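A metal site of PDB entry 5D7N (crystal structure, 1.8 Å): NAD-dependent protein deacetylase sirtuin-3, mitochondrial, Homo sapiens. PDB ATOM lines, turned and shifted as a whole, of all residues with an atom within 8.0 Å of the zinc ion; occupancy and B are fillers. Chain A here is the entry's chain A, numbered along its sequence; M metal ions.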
ATOM      1  N   THR A 141       3.815  31.302  18.578  1.00  0.00           N
ATOM      2  CA  THR A 141       2.423  31.403  19.040  1.00  0.00           C
ATOM      3  C   THR A 141       1.518  30.577  18.123  1.00  0.00           C
ATOM      4  O   THR A 141       1.639  30.641  16.895  1.00  0.00           O
ATOM      5  CB  THR A 141       1.951  32.868  19.016  1.00  0.00           C
ATOM      6  OG1 THR A 141       2.811  33.658  19.837  1.00  0.00           O
ATOM      7  CG2 THR A 141       0.510  33.026  19.527  1.00  0.00           C
ATOM      8  N   CYS A 142       0.631  29.793  18.731  1.00  0.00           N
ATOM      9  CA  CYS A 142      -0.344  29.013  17.978  1.00  0.00           C
ATOM     10  C   CYS A 142      -1.272  29.963  17.270  1.00  0.00           C
ATOM     11  O   CYS A 142      -1.829  30.867  17.893  1.00  0.00           O
ATOM     12  CB  CYS A 142      -1.143  28.076  18.861  1.00  0.00           C
ATOM     13  SG  CYS A 142      -2.373  27.150  17.906  1.00  0.00           S
ATOM     14  N   THR A 143      -1.408  29.770  15.975  1.00  0.00           N
ATOM     15  CA  THR A 143      -2.214  30.638  15.125  1.00  0.00           C
ATOM     16  C   THR A 143      -3.707  30.473  15.416  1.00  0.00           C
ATOM     17  O   THR A 143      -4.485  31.342  15.051  1.00  0.00           O
ATOM     18  CB  THR A 143      -1.992  30.360  13.631  1.00  0.00           C
ATOM     19  OG1 THR A 143      -2.242  28.984  13.330  1.00  0.00           O
ATOM     20  CG2 THR A 143      -0.555  30.731  13.197  1.00  0.00           C
ATOM     21  N   VAL A 144      -4.089  29.394  16.092  1.00  0.00           N
ATOM     22  CA  VAL A 144      -5.501  29.105  16.362  1.00  0.00           C
ATOM     23  C   VAL A 144      -5.843  29.477  17.800  1.00  0.00           C
ATOM     24  O   VAL A 144      -6.682  30.335  18.018  1.00  0.00           O
ATOM     25  CB  VAL A 144      -5.843  27.623  16.073  1.00  0.00           C
ATOM     26  CG1 VAL A 144      -7.225  27.237  16.602  1.00  0.00           C
ATOM     27  CG2 VAL A 144      -5.750  27.358  14.597  1.00  0.00           C
ATOM     28  N   CYS A 145      -5.194  28.870  18.784  1.00  0.00           N
ATOM     29  CA  CYS A 145      -5.560  29.117  20.181  1.00  0.00           C
ATOM     30  C   CYS A 145      -4.731  30.189  20.879  1.00  0.00           C
ATOM     31  O   CYS A 145      -5.000  30.510  22.033  1.00  0.00           O
ATOM     32  CB  CYS A 145      -5.512  27.821  20.992  1.00  0.00           C
ATOM     33  SG  CYS A 145      -3.847  27.282  21.374  1.00  0.00           S
ATOM     34  N   GLN A 146      -3.719  30.725  20.204  1.00  0.00           N
ATOM     35  CA  GLN A 146      -2.899  31.817  20.736  1.00  0.00           C
ATOM     36  C   GLN A 146      -2.006  31.431  21.918  1.00  0.00           C
ATOM     37  O   GLN A 146      -1.472  32.312  22.581  1.00  0.00           O
ATOM     38  CB  GLN A 146      -3.761  33.035  21.131  1.00  0.00           C
ATOM     39  CG  GLN A 146      -4.781  33.459  20.088  1.00  0.00           C
ATOM     40  CD  GLN A 146      -4.162  33.554  18.728  1.00  0.00           C
ATOM     41  OE1 GLN A 146      -3.116  34.171  18.572  1.00  0.00           O
ATOM     42  NE2 GLN A 146      -4.786  32.922  17.726  1.00  0.00           N
ATOM     43  N   ARG A 147      -1.806  30.138  22.151  1.00  0.00           N
ATOM     44  CA  ARG A 147      -0.839  29.705  23.177  1.00  0.00           C
ATOM     45  C   ARG A 147       0.581  30.068  22.751  1.00  0.00           C
ATOM     46  O   ARG A 147       0.949  29.828  21.600  1.00  0.00           O
ATOM     47  CB  ARG A 147      -0.938  28.203  23.421  1.00  0.00           C
ATOM     48  CG  ARG A 147      -1.964  27.859  24.498  1.00  0.00           C
ATOM     49  CD  ARG A 147      -2.252  26.373  24.597  1.00  0.00           C
ATOM     50  NE  ARG A 147      -3.271  26.136  25.617  1.00  0.00           N
ATOM     51  CZ  ARG A 147      -4.584  26.188  25.429  1.00  0.00           C
ATOM     52  NH1 ARG A 147      -5.096  26.458  24.229  1.00  0.00           N
ATOM     53  NH2 ARG A 147      -5.404  25.972  26.454  1.00  0.00           N
ATOM     54  N   PRO A 148       1.368  30.652  23.674  1.00  0.00           N
ATOM     55  CA  PRO A 148       2.784  30.941  23.437  1.00  0.00           C
ATOM     56  C   PRO A 148       3.662  29.731  23.699  1.00  0.00           C
ATOM     57  O   PRO A 148       3.351  28.925  24.565  1.00  0.00           O
ATOM     58  CB  PRO A 148       3.088  32.058  24.447  1.00  0.00           C
ATOM     59  CG  PRO A 148       2.135  31.817  25.568  1.00  0.00           C
ATOM     60  CD  PRO A 148       0.892  31.246  24.947  1.00  0.00           C
ATOM     61  N   PHE A 149       4.755  29.596  22.950  1.00  0.00           N
ATOM     62  CA  PHE A 149       5.729  28.525  23.167  1.00  0.00           C
ATOM     63  C   PHE A 149       7.147  29.056  22.957  1.00  0.00           C
ATOM     64  O   PHE A 149       7.359  30.000  22.182  1.00  0.00           O
ATOM     65  CB  PHE A 149       5.495  27.372  22.192  1.00  0.00           C
ATOM     66  CG  PHE A 149       4.132  26.780  22.268  1.00  0.00           C
ATOM     67  CD1 PHE A 149       3.818  25.848  23.255  1.00  0.00           C
ATOM     68  CD2 PHE A 149       3.129  27.172  21.372  1.00  0.00           C
ATOM     69  CE1 PHE A 149       2.538  25.306  23.348  1.00  0.00           C
ATOM     70  CE2 PHE A 149       1.857  26.633  21.461  1.00  0.00           C
ATOM     71  CZ  PHE A 149       1.568  25.698  22.446  1.00  0.00           C
ATOM     72  N   ARG A 165       2.838  21.986  14.693  1.00  0.00           N
ATOM     73  CA  ARG A 165       1.437  22.070  15.099  1.00  0.00           C
ATOM     74  C   ARG A 165       1.253  22.091  16.610  1.00  0.00           C
ATOM     75  O   ARG A 165       2.047  21.521  17.341  1.00  0.00           O
ATOM     76  CB  ARG A 165       0.661  20.955  14.444  1.00  0.00           C
ATOM     77  CG  ARG A 165       0.612  21.107  12.934  1.00  0.00           C
ATOM     78  CD  ARG A 165      -0.145  19.990  12.268  1.00  0.00           C
ATOM     79  NE  ARG A 165      -1.562  20.020  12.593  1.00  0.00           N
ATOM     80  CZ  ARG A 165      -2.446  19.170  12.103  1.00  0.00           C
ATOM     81  NH1 ARG A 165      -2.057  18.213  11.266  1.00  0.00           N
ATOM     82  NH2 ARG A 165      -3.726  19.242  12.449  1.00  0.00           N
ATOM     83  N   CYS A 166       0.219  22.794  17.068  1.00  0.00           N
ATOM     84  CA  CYS A 166       0.006  23.022  18.490  1.00  0.00           C
ATOM     85  C   CYS A 166      -0.363  21.724  19.216  1.00  0.00           C
ATOM     86  O   CYS A 166      -1.207  20.967  18.741  1.00  0.00           O
ATOM     87  CB  CYS A 166      -1.130  23.997  18.631  1.00  0.00           C
ATOM     88  SG  CYS A 166      -1.619  24.410  20.313  1.00  0.00           S
ATOM     89  N   PRO A 167       0.253  21.466  20.369  1.00  0.00           N
ATOM     90  CA  PRO A 167      -0.089  20.225  21.077  1.00  0.00           C
ATOM     91  C   PRO A 167      -1.484  20.219  21.699  1.00  0.00           C
ATOM     92  O   PRO A 167      -1.950  19.162  22.135  1.00  0.00           O
ATOM     93  CB  PRO A 167       0.967  20.140  22.179  1.00  0.00           C
ATOM     94  CG  PRO A 167       1.417  21.553  22.406  1.00  0.00           C
ATOM     95  CD  PRO A 167       1.289  22.246  21.075  1.00  0.00           C
ATOM     96  N   VAL A 168      -2.142  21.379  21.780  1.00  0.00           N
ATOM     97  CA  VAL A 168      -3.476  21.487  22.338  1.00  0.00           C
ATOM     98  C   VAL A 168      -4.527  21.408  21.242  1.00  0.00           C
ATOM     99  O   VAL A 168      -5.380  20.532  21.290  1.00  0.00           O
ATOM    100  CB  VAL A 168      -3.635  22.772  23.201  1.00  0.00           C
ATOM    101  CG1 VAL A 168      -5.081  22.967  23.662  1.00  0.00           C
ATOM    102  CG2 VAL A 168      -2.728  22.731  24.407  1.00  0.00           C
ATOM    103  N   CYS A 169      -4.461  22.294  20.250  1.00  0.00           N
ATOM    104  CA  CYS A 169      -5.525  22.391  19.237  1.00  0.00           C
ATOM    105  C   CYS A 169      -5.105  21.905  17.852  1.00  0.00           C
ATOM    106  O   CYS A 169      -5.935  21.823  16.954  1.00  0.00           O
ATOM    107  CB  CYS A 169      -5.996  23.836  19.174  1.00  0.00           C
ATOM    108  SG  CYS A 169      -4.889  24.936  18.256  1.00  0.00           S
ATOM    109  N   THR A 170      -3.831  21.565  17.687  1.00  0.00           N
ATOM    110  CA  THR A 170      -3.199  21.149  16.401  1.00  0.00           C
ATOM    111  C   THR A 170      -3.041  22.260  15.335  1.00  0.00           C
ATOM    112  O   THR A 170      -2.617  21.982  14.214  1.00  0.00           O
ATOM    113  CB  THR A 170      -3.871  19.907  15.794  1.00  0.00           C
ATOM    114  OG1 THR A 170      -5.083  20.279  15.110  1.00  0.00           O
ATOM    115  CG2 THR A 170      -4.197  18.881  16.889  1.00  0.00           C
ATOM    116  N   GLY A 171      -3.325  23.505  15.679  1.00  0.00           N
ATOM    117  CA  GLY A 171      -3.151  24.621  14.744  1.00  0.00           C
ATOM    118  C   GLY A 171      -1.677  24.854  14.429  1.00  0.00           C
ATOM    119  O   GLY A 171      -0.816  24.378  15.160  1.00  0.00           O
ATOM    120  N   VAL A 172      -1.383  25.562  13.347  1.00  0.00           N
ATOM    121  CA  VAL A 172       0.016  25.849  13.003  1.00  0.00           C
ATOM    122  C   VAL A 172       0.614  26.755  14.076  1.00  0.00           C
ATOM    123  O   VAL A 172      -0.029  27.724  14.491  1.00  0.00           O
ATOM    124  CB  VAL A 172       0.173  26.535  11.634  1.00  0.00           C
ATOM    125  CG1 VAL A 172       1.640  26.927  11.396  1.00  0.00           C
ATOM    126  CG2 VAL A 172      -0.301  25.618  10.534  1.00  0.00           C
ATOM    127  N   VAL A 173       1.802  26.413  14.546  1.00  0.00           N
ATOM    128  CA  VAL A 173       2.545  27.236  15.498  1.00  0.00           C
ATOM    129  C   VAL A 173       3.519  28.113  14.715  1.00  0.00           C
ATOM    130  O   VAL A 173       4.417  27.605  14.040  1.00  0.00           O
ATOM    131  CB  VAL A 173       3.294  26.372  16.522  1.00  0.00           C
ATOM    132  CG1 VAL A 173       4.207  27.222  17.404  1.00  0.00           C
ATOM    133  CG2 VAL A 173       2.301  25.596  17.380  1.00  0.00           C
HETATM  134 ZN    ZN M   1      -3.253  25.862  19.630  1.00  0.00          ZN
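The zinc ion is bound by SG of Cys 166 (2.3 Å), SG of Cys 142 (2.3 Å), SG of Cys 145 (2.3 Å) and SG of Cys 169 (2.3 Å).
The backbone NH (N) of Cys 142 lies within hydrogen-bond range of the backbone carbonyl oxygen (O) of Arg 147 (2.9 Å). SG of Cys 142 lies close to N of Val 144. N of Val 168 lies close to SG of Cys 166 (3.4 Å). The backbone NH of Cys 166 sits at hydrogen-bond distance from the backbone carbonyl oxygen of Gly 171, 2.7 Å away. The guanidinium group (NH1) of Arg 147 lies close to the side-chain sulfur (SG) of Cys 145 (3.2 Å). N of Gly 171 sits close to SG of Cys 169 (3.3 Å).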
